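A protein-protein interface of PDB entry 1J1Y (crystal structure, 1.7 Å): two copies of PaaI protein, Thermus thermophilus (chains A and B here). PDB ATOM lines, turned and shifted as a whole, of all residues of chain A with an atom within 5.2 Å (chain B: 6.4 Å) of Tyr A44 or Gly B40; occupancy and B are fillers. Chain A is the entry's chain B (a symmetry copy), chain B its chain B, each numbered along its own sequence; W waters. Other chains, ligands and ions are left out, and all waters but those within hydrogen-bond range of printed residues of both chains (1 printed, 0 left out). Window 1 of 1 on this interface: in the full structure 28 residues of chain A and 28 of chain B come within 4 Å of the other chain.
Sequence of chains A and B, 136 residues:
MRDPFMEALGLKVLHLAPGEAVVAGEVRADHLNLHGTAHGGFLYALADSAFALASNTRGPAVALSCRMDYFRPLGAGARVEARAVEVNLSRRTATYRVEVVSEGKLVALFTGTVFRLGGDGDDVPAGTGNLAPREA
A ring nitrogen (ND1) of His B39 lies close to the side-chain carboxylate (OD2) of Asp A48, 3.5 Å away.
A ring nitrogen (NE2) of His B39 lies within hydrogen-bond range of the side-chain hydroxyl of Ser A49, 3.3 Å away.
The side-chain hydroxyl (OH) of Tyr B44 sits at hydrogen-bond distance from the side-chain hydroxyl (OH) of Tyr A70 (2.8 Å).
The backbone carbonyl oxygen (O) of Cys B66 lies within hydrogen-bond range of the backbone NH (N) of Met A68 (2.8 Å).
The backbone NH of Met B68 sits at hydrogen-bond distance from the backbone carbonyl oxygen of Cys A66 (2.8 Å).
The side-chain hydroxyl (OH) of Tyr B70 sits at hydrogen-bond distance from the side-chain hydroxyl (OH) of Tyr A44 (2.8 Å).
Of the 14 printed residues of chain B, 7 touch a printed residue of chain A.
Hydrophobic or aromatic side chains of chain B that line the printed part of chain A: His B39, Tyr B44, Met B68 and Tyr B70.
Of the 14 printed residues of chain A, 7 touch a printed residue of chain B.
Among the printed residues, 14 pairs touch across the chains.
Tyr A44 touches just these residues of chain B: Gly B40, Tyr B44, Met B68 and Tyr B70.
Gly B40 touches just these residues of chain A: Tyr A44 and Asp A48.
Printed residues of chain A within 4 Å of His B39: Asp A48 and Ser A49.
Of the printed residues of chain A, Gly B41 touches Asp A48.
Printed residues of chain B within 4 Å of Asp A48: His B39 (3.1 Å), Gly B40 (3.7 Å) and Gly B41 (3.5 Å).
The nearest printed residue of chain A that does not touch Gly B40 is Ala A45 (6.2 Å).
The nearest printed residue of chain B that does not touch Gly A40 is Ala B45 (6.2 Å).
Water W1 lies within hydrogen-bond range of OD2 of Asp A48 (2.7 Å) and N of Gly B40 (3.0 Å).
The backbone NH (N) of His B39 lies within hydrogen-bond range of the backbone carbonyl oxygen (O) of His B31 (2.9 Å).
N of Gly B41 lies within hydrogen-bond range of ND1 of His B39 (2.8 Å).
The side-chain hydroxyl (OH) of Tyr B70 sits at hydrogen-bond distance from the backbone carbonyl oxygen (O) of Gly B40, at 2.8 Å.
The side-chain sulfur (SG) of Cys B66 sits close to the side-chain hydroxyl (OH) of Tyr B44, 3.6 Å away.
The side-chain hydroxyl (OH) of Tyr A44 sits close to the side-chain sulfur (SG) of Cys A66.
O of Ala A45 sits at hydrogen-bond distance from OG of Ser A49 (2.8 Å).
CE1 of Tyr B44 touches O of Gly A40, 3.8 Å away.
Tyr A44 touches Gly B40 (CE1 to O, 3.8 Å).
CE2 of Tyr B44 touches CD2 of Tyr A44, 3.3 Å away.
Tyr A44 touches Met B68.
CA of Gly B40 touches OD2 of Asp A48, 3.7 Å away.
Asp A48 touches Gly B41.
Cys A66 touches Cys B66 (O to O, 3.9 Å).
Met A68 touches Tyr B44.
Gly A40 touches Tyr B44, and with the chains exchanged Tyr A44 touches Gly B40.
Tyr B44 touches its own counterpart, Tyr A44.
Tyr A44 touches Met B68, and with the chains exchanged Met A68 touches Tyr B44.
Tyr A44 touches Tyr B70, and with the chains exchanged Tyr A70 touches Tyr B44.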
ATOM      1  N   GLY A  40      -1.812  20.577  12.405  1.00  0.00           N
ATOM      2  CA  GLY A  40      -1.704  19.186  12.808  1.00  0.00           C
ATOM      3  C   GLY A  40      -2.305  18.239  11.786  1.00  0.00           C
ATOM      4  O   GLY A  40      -1.862  17.098  11.640  1.00  0.00           O
ATOM      5  N   GLY A  41      -3.320  18.716  11.075  1.00  0.00           N
ATOM      6  CA  GLY A  41      -3.969  17.901  10.064  1.00  0.00           C
ATOM      7  C   GLY A  41      -3.099  17.640   8.849  1.00  0.00           C
ATOM      8  O   GLY A  41      -3.242  16.609   8.185  1.00  0.00           O
ATOM      9  N   PHE A  42      -2.203  18.571   8.541  1.00  0.00           N
ATOM     10  CA  PHE A  42      -1.320  18.394   7.396  1.00  0.00           C
ATOM     11  C   PHE A  42      -0.284  17.323   7.714  1.00  0.00           C
ATOM     12  O   PHE A  42      -0.049  16.415   6.919  1.00  0.00           O
ATOM     13  CB  PHE A  42      -0.603  19.701   7.043  1.00  0.00           C
ATOM     14  CG  PHE A  42       0.402  19.545   5.941  1.00  0.00           C
ATOM     15  CD1 PHE A  42      -0.012  19.271   4.641  1.00  0.00           C
ATOM     16  CD2 PHE A  42       1.765  19.599   6.213  1.00  0.00           C
ATOM     17  CE1 PHE A  42       0.918  19.046   3.627  1.00  0.00           C
ATOM     18  CE2 PHE A  42       2.702  19.376   5.205  1.00  0.00           C
ATOM     19  CZ  PHE A  42       2.282  19.099   3.915  1.00  0.00           C
ATOM     20  N   LEU A  43       0.339  17.429   8.883  1.00  0.00           N
ATOM     21  CA  LEU A  43       1.341  16.445   9.270  1.00  0.00           C
ATOM     22  C   LEU A  43       0.713  15.064   9.382  1.00  0.00           C
ATOM     23  O   LEU A  43       1.321  14.063   8.996  1.00  0.00           O
ATOM     24  CB  LEU A  43       2.003  16.845  10.592  1.00  0.00           C
ATOM     25  CG  LEU A  43       2.839  18.124  10.511  1.00  0.00           C
ATOM     26  CD1 LEU A  43       3.501  18.386  11.852  1.00  0.00           C
ATOM     27  CD2 LEU A  43       3.894  17.978   9.418  1.00  0.00           C
ATOM     28  N   TYR A  44      -0.511  15.000   9.899  1.00  0.00           N
ATOM     29  CA  TYR A  44      -1.185  13.718  10.008  1.00  0.00           C
ATOM     30  C   TYR A  44      -1.522  13.181   8.619  1.00  0.00           C
ATOM     31  O   TYR A  44      -1.365  11.992   8.352  1.00  0.00           O
ATOM     32  CB  TYR A  44      -2.457  13.852  10.846  1.00  0.00           C
ATOM     33  CG  TYR A  44      -3.222  12.559  10.995  1.00  0.00           C
ATOM     34  CD1 TYR A  44      -4.073  12.104   9.983  1.00  0.00           C
ATOM     35  CD2 TYR A  44      -3.099  11.790  12.149  1.00  0.00           C
ATOM     36  CE1 TYR A  44      -4.787  10.918  10.122  1.00  0.00           C
ATOM     37  CE2 TYR A  44      -3.806  10.603  12.297  1.00  0.00           C
ATOM     38  CZ  TYR A  44      -4.647  10.174  11.285  1.00  0.00           C
ATOM     39  OH  TYR A  44      -5.361   9.004  11.445  1.00  0.00           O
ATOM     40  N   ALA A  45      -1.977  14.055   7.725  1.00  0.00           N
ATOM     41  CA  ALA A  45      -2.322  13.618   6.377  1.00  0.00           C
ATOM     42  C   ALA A  45      -1.104  12.994   5.708  1.00  0.00           C
ATOM     43  O   ALA A  45      -1.216  11.991   5.007  1.00  0.00           O
ATOM     44  CB  ALA A  45      -2.830  14.794   5.552  1.00  0.00           C
ATOM     45  N   LEU A  46       0.060  13.591   5.940  1.00  0.00           N
ATOM     46  CA  LEU A  46       1.305  13.090   5.373  1.00  0.00           C
ATOM     47  C   LEU A  46       1.608  11.691   5.903  1.00  0.00           C
ATOM     48  O   LEU A  46       1.853  10.758   5.133  1.00  0.00           O
ATOM     49  CB  LEU A  46       2.459  14.027   5.730  1.00  0.00           C
ATOM     50  CG  LEU A  46       3.837  13.530   5.297  1.00  0.00           C
ATOM     51  CD1 LEU A  46       4.014  13.765   3.806  1.00  0.00           C
ATOM     52  CD2 LEU A  46       4.913  14.265   6.074  1.00  0.00           C
ATOM     53  N   ALA A  47       1.579  11.546   7.223  1.00  0.00           N
ATOM     54  CA  ALA A  47       1.863  10.259   7.850  1.00  0.00           C
ATOM     55  C   ALA A  47       0.833   9.210   7.452  1.00  0.00           C
ATOM     56  O   ALA A  47       1.174   8.067   7.143  1.00  0.00           O
ATOM     57  CB  ALA A  47       1.895  10.414   9.365  1.00  0.00           C
ATOM     58  N   ASP A  48      -0.433   9.613   7.461  1.00  0.00           N
ATOM     59  CA  ASP A  48      -1.525   8.723   7.106  1.00  0.00           C
ATOM     60  C   ASP A  48      -1.390   8.232   5.668  1.00  0.00           C
ATOM     61  O   ASP A  48      -1.727   7.089   5.362  1.00  0.00           O
ATOM     62  CB  ASP A  48      -2.858   9.449   7.283  1.00  0.00           C
ATOM     63  CG  ASP A  48      -4.043   8.534   7.105  1.00  0.00           C
ATOM     64  OD1 ASP A  48      -4.272   7.673   7.986  1.00  0.00           O
ATOM     65  OD2 ASP A  48      -4.743   8.670   6.083  1.00  0.00           O
ATOM     66  N   SER A  49      -0.901   9.095   4.782  1.00  0.00           N
ATOM     67  CA  SER A  49      -0.732   8.703   3.386  1.00  0.00           C
ATOM     68  C   SER A  49       0.331   7.617   3.247  1.00  0.00           C
ATOM     69  O   SER A  49       0.150   6.664   2.492  1.00  0.00           O
ATOM     70  CB  SER A  49      -0.364   9.913   2.526  1.00  0.00           C
ATOM     71  OG  SER A  49      -1.447  10.829   2.480  1.00  0.00           O
ATOM     72  N   CYS A  66      -5.562   5.179  14.764  1.00  0.00           N
ATOM     73  CA  CYS A  66      -4.258   5.796  14.558  1.00  0.00           C
ATOM     74  C   CYS A  66      -3.929   6.786  15.666  1.00  0.00           C
ATOM     75  O   CYS A  66      -4.816   7.445  16.206  1.00  0.00           O
ATOM     76  CB  CYS A  66      -4.230   6.533  13.219  1.00  0.00           C
ATOM     77  SG  CYS A  66      -4.716   5.520  11.810  1.00  0.00           S
ATOM     78  N   MET A  68      -1.159   9.988  16.747  1.00  0.00           N
ATOM     79  CA  MET A  68      -0.193  10.946  16.246  1.00  0.00           C
ATOM     80  C   MET A  68       0.407  11.700  17.426  1.00  0.00           C
ATOM     81  O   MET A  68      -0.314  12.310  18.216  1.00  0.00           O
ATOM     82  CB  MET A  68      -0.870  11.928  15.292  1.00  0.00           C
ATOM     83  CG  MET A  68       0.068  12.947  14.705  1.00  0.00           C
ATOM     84  SD  MET A  68       1.107  12.234  13.426  1.00  0.00           S
ATOM     85  CE  MET A  68       1.579  13.706  12.570  1.00  0.00           C
ATOM     86  N   TYR A  70       3.044  14.659  18.384  1.00  0.00           N
ATOM     87  CA  TYR A  70       3.734  15.837  17.847  1.00  0.00           C
ATOM     88  C   TYR A  70       4.911  16.259  18.720  1.00  0.00           C
ATOM     89  O   TYR A  70       4.757  16.427  19.933  1.00  0.00           O
ATOM     90  CB  TYR A  70       2.733  16.989  17.740  1.00  0.00           C
ATOM     91  CG  TYR A  70       1.576  16.702  16.810  1.00  0.00           C
ATOM     92  CD1 TYR A  70       1.700  16.893  15.434  1.00  0.00           C
ATOM     93  CD2 TYR A  70       0.352  16.247  17.306  1.00  0.00           C
ATOM     94  CE1 TYR A  70       0.632  16.639  14.571  1.00  0.00           C
ATOM     95  CE2 TYR A  70      -0.723  15.993  16.450  1.00  0.00           C
ATOM     96  CZ  TYR A  70      -0.574  16.193  15.087  1.00  0.00           C
ATOM     97  OH  TYR A  70      -1.637  15.959  14.241  1.00  0.00           O
ATOM     98  N   PHE A 110       3.748   8.570  14.207  1.00  0.00           N
ATOM     99  CA  PHE A 110       2.418   8.066  13.893  1.00  0.00           C
ATOM    100  C   PHE A 110       2.378   6.551  14.079  1.00  0.00           C
ATOM    101  O   PHE A 110       3.306   5.838  13.694  1.00  0.00           O
ATOM    102  CB  PHE A 110       2.085   8.460  12.442  1.00  0.00           C
ATOM    103  CG  PHE A 110       0.813   7.858  11.899  1.00  0.00           C
ATOM    104  CD1 PHE A 110       0.752   6.508  11.555  1.00  0.00           C
ATOM    105  CD2 PHE A 110      -0.304   8.658  11.674  1.00  0.00           C
ATOM    106  CE1 PHE A 110      -0.402   5.965  10.990  1.00  0.00           C
ATOM    107  CE2 PHE A 110      -1.466   8.126  11.107  1.00  0.00           C
ATOM    108  CZ  PHE A 110      -1.512   6.779  10.764  1.00  0.00           C
ATOM    109  N   HIS B  31     -10.706  15.482  -1.652  1.00  0.00           N
ATOM    110  CA  HIS B  31     -10.562  14.922  -0.304  1.00  0.00           C
ATOM    111  C   HIS B  31     -10.637  13.403  -0.316  1.00  0.00           C
ATOM    112  O   HIS B  31     -10.583  12.763   0.735  1.00  0.00           O
ATOM    113  CB  HIS B  31     -11.666  15.466   0.607  1.00  0.00           C
ATOM    114  CG  HIS B  31     -11.632  16.952   0.762  1.00  0.00           C
ATOM    115  ND1 HIS B  31     -12.757  17.699   1.037  1.00  0.00           N
ATOM    116  CD2 HIS B  31     -10.604  17.830   0.694  1.00  0.00           C
ATOM    117  CE1 HIS B  31     -12.423  18.974   1.133  1.00  0.00           C
ATOM    118  NE2 HIS B  31     -11.122  19.080   0.929  1.00  0.00           N
ATOM    119  N   ASN B  33      -9.469   9.434  -1.319  1.00  0.00           N
ATOM    120  CA  ASN B  33      -8.243   8.655  -1.408  1.00  0.00           C
ATOM    121  C   ASN B  33      -8.321   7.888  -2.725  1.00  0.00           C
ATOM    122  O   ASN B  33      -9.311   7.991  -3.449  1.00  0.00           O
ATOM    123  CB  ASN B  33      -8.125   7.680  -0.232  1.00  0.00           C
ATOM    124  CG  ASN B  33      -9.368   6.833  -0.047  1.00  0.00           C
ATOM    125  OD1 ASN B  33      -9.983   6.397  -1.016  1.00  0.00           O
ATOM    126  ND2 ASN B  33      -9.734   6.587   1.206  1.00  0.00           N
ATOM    127  N   THR B  37     -13.047   6.884  -1.325  1.00  0.00           N
ATOM    128  CA  THR B  37     -13.736   7.324  -0.114  1.00  0.00           C
ATOM    129  C   THR B  37     -12.951   8.453   0.542  1.00  0.00           C
ATOM    130  O   THR B  37     -11.828   8.753   0.135  1.00  0.00           O
ATOM    131  CB  THR B  37     -13.899   6.172   0.905  1.00  0.00           C
ATOM    132  OG1 THR B  37     -12.615   5.616   1.217  1.00  0.00           O
ATOM    133  CG2 THR B  37     -14.796   5.081   0.337  1.00  0.00           C
ATOM    134  N   ALA B  38     -13.546   9.082   1.549  1.00  0.00           N
ATOM    135  CA  ALA B  38     -12.891  10.178   2.248  1.00  0.00           C
ATOM    136  C   ALA B  38     -11.556   9.722   2.827  1.00  0.00           C
ATOM    137  O   ALA B  38     -11.484   8.713   3.530  1.00  0.00           O
ATOM    138  CB  ALA B  38     -13.790  10.702   3.359  1.00  0.00           C
ATOM    139  N   HIS B  39     -10.503  10.474   2.520  1.00  0.00           N
ATOM    140  CA  HIS B  39      -9.161  10.163   2.998  1.00  0.00           C
ATOM    141  C   HIS B  39      -9.125  10.323   4.515  1.00  0.00           C
ATOM    142  O   HIS B  39      -9.749  11.233   5.066  1.00  0.00           O
ATOM    143  CB  HIS B  39      -8.155  11.110   2.329  1.00  0.00           C
ATOM    144  CG  HIS B  39      -6.722  10.714   2.505  1.00  0.00           C
ATOM    145  ND1 HIS B  39      -6.047  10.861   3.698  1.00  0.00           N
ATOM    146  CD2 HIS B  39      -5.828  10.194   1.629  1.00  0.00           C
ATOM    147  CE1 HIS B  39      -4.800  10.449   3.550  1.00  0.00           C
ATOM    148  NE2 HIS B  39      -4.641  10.040   2.304  1.00  0.00           N
ATOM    149  N   GLY B  40      -8.404   9.429   5.187  1.00  0.00           N
ATOM    150  CA  GLY B  40      -8.303   9.499   6.635  1.00  0.00           C
ATOM    151  C   GLY B  40      -7.763  10.833   7.114  1.00  0.00           C
ATOM    152  O   GLY B  40      -8.099  11.300   8.204  1.00  0.00           O
ATOM    153  N   GLY B  41      -6.922  11.451   6.292  1.00  0.00           N
ATOM    154  CA  GLY B  41      -6.347  12.737   6.644  1.00  0.00           C
ATOM    155  C   GLY B  41      -7.355  13.871   6.638  1.00  0.00           C
ATOM    156  O   GLY B  41      -7.204  14.849   7.375  1.00  0.00           O
ATOM    157  N   PHE B  42      -8.381  13.758   5.801  1.00  0.00           N
ATOM    158  CA  PHE B  42      -9.400  14.796   5.740  1.00  0.00           C
ATOM    159  C   PHE B  42     -10.258  14.741   6.998  1.00  0.00           C
ATOM    160  O   PHE B  42     -10.510  15.762   7.635  1.00  0.00           O
ATOM    161  CB  PHE B  42     -10.295  14.620   4.509  1.00  0.00           C
ATOM    162  CG  PHE B  42     -11.431  15.598   4.460  1.00  0.00           C
ATOM    163  CD1 PHE B  42     -11.188  16.953   4.249  1.00  0.00           C
ATOM    164  CD2 PHE B  42     -12.737  15.180   4.697  1.00  0.00           C
ATOM    165  CE1 PHE B  42     -12.229  17.879   4.280  1.00  0.00           C
ATOM    166  CE2 PHE B  42     -13.784  16.100   4.730  1.00  0.00           C
ATOM    167  CZ  PHE B  42     -13.533  17.447   4.523  1.00  0.00           C
ATOM    168  N   LEU B  43     -10.707  13.543   7.357  1.00  0.00           N
ATOM    169  CA  LEU B  43     -11.531  13.399   8.550  1.00  0.00           C
ATOM    170  C   LEU B  43     -10.750  13.817   9.787  1.00  0.00           C
ATOM    171  O   LEU B  43     -11.300  14.444  10.695  1.00  0.00           O
ATOM    172  CB  LEU B  43     -12.028  11.957   8.687  1.00  0.00           C
ATOM    173  CG  LEU B  43     -12.997  11.522   7.586  1.00  0.00           C
ATOM    174  CD1 LEU B  43     -13.478  10.107   7.858  1.00  0.00           C
ATOM    175  CD2 LEU B  43     -14.182  12.484   7.538  1.00  0.00           C
ATOM    176  N   TYR B  44      -9.463  13.482   9.827  1.00  0.00           N
ATOM    177  CA  TYR B  44      -8.649  13.874  10.964  1.00  0.00           C
ATOM    178  C   TYR B  44      -8.466  15.391  10.983  1.00  0.00           C
ATOM    179  O   TYR B  44      -8.534  16.016  12.037  1.00  0.00           O
ATOM    180  CB  TYR B  44      -7.288  13.179  10.912  1.00  0.00           C
ATOM    181  CG  TYR B  44      -6.376  13.548  12.057  1.00  0.00           C
ATOM    182  CD1 TYR B  44      -5.642  14.737  12.041  1.00  0.00           C
ATOM    183  CD2 TYR B  44      -6.245  12.705  13.159  1.00  0.00           C
ATOM    184  CE1 TYR B  44      -4.794  15.074  13.091  1.00  0.00           C
ATOM    185  CE2 TYR B  44      -5.401  13.033  14.213  1.00  0.00           C
ATOM    186  CZ  TYR B  44      -4.679  14.214  14.174  1.00  0.00           C
ATOM    187  OH  TYR B  44      -3.829  14.525  15.216  1.00  0.00           O
ATOM    188  N   ALA B  45      -8.245  15.989   9.816  1.00  0.00           N
ATOM    189  CA  ALA B  45      -8.060  17.434   9.752  1.00  0.00           C
ATOM    190  C   ALA B  45      -9.290  18.138  10.309  1.00  0.00           C
ATOM    191  O   ALA B  45      -9.178  19.139  11.013  1.00  0.00           O
ATOM    192  CB  ALA B  45      -7.807  17.874   8.314  1.00  0.00           C
ATOM    193  N   CYS B  66      -2.733  12.695  19.813  1.00  0.00           N
ATOM    194  CA  CYS B  66      -4.111  12.547  19.364  1.00  0.00           C
ATOM    195  C   CYS B  66      -4.375  11.145  18.830  1.00  0.00           C
ATOM    196  O   CYS B  66      -3.493  10.516  18.250  1.00  0.00           O
ATOM    197  CB  CYS B  66      -4.416  13.556  18.257  1.00  0.00           C
ATOM    198  SG  CYS B  66      -4.040  15.264  18.694  1.00  0.00           S
ATOM    199  N   MET B  68      -7.278   8.781  16.577  1.00  0.00           N
ATOM    200  CA  MET B  68      -8.404   8.833  15.666  1.00  0.00           C
ATOM    201  C   MET B  68      -8.898   7.414  15.416  1.00  0.00           C
ATOM    202  O   MET B  68      -8.136   6.548  14.984  1.00  0.00           O
ATOM    203  CB  MET B  68      -7.983   9.476  14.345  1.00  0.00           C
ATOM    204  CG  MET B  68      -9.101   9.590  13.345  1.00  0.00           C
ATOM    205  SD  MET B  68     -10.237  10.915  13.767  1.00  0.00           S
ATOM    206  CE  MET B  68     -10.985  11.182  12.188  1.00  0.00           C
ATOM    207  N   TYR B  70     -11.663   5.259  13.332  1.00  0.00           N
ATOM    208  CA  TYR B  70     -12.546   5.300  12.162  1.00  0.00           C
ATOM    209  C   TYR B  70     -13.618   4.217  12.214  1.00  0.00           C
ATOM    210  O   TYR B  70     -13.304   3.041  12.413  1.00  0.00           O
ATOM    211  CB  TYR B  70     -11.699   5.127  10.899  1.00  0.00           C
ATOM    212  CG  TYR B  70     -10.669   6.217  10.705  1.00  0.00           C
ATOM    213  CD1 TYR B  70     -11.016   7.431  10.114  1.00  0.00           C
ATOM    214  CD2 TYR B  70      -9.344   6.031  11.105  1.00  0.00           C
ATOM    215  CE1 TYR B  70     -10.067   8.437   9.923  1.00  0.00           C
ATOM    216  CE2 TYR B  70      -8.387   7.032  10.916  1.00  0.00           C
ATOM    217  CZ  TYR B  70      -8.757   8.229  10.323  1.00  0.00           C
ATOM    218  OH  TYR B  70      -7.813   9.212  10.120  1.00  0.00           O
HETATM  219  O   HOH W   1      -6.414   7.332   4.378  1.00  0.00           O
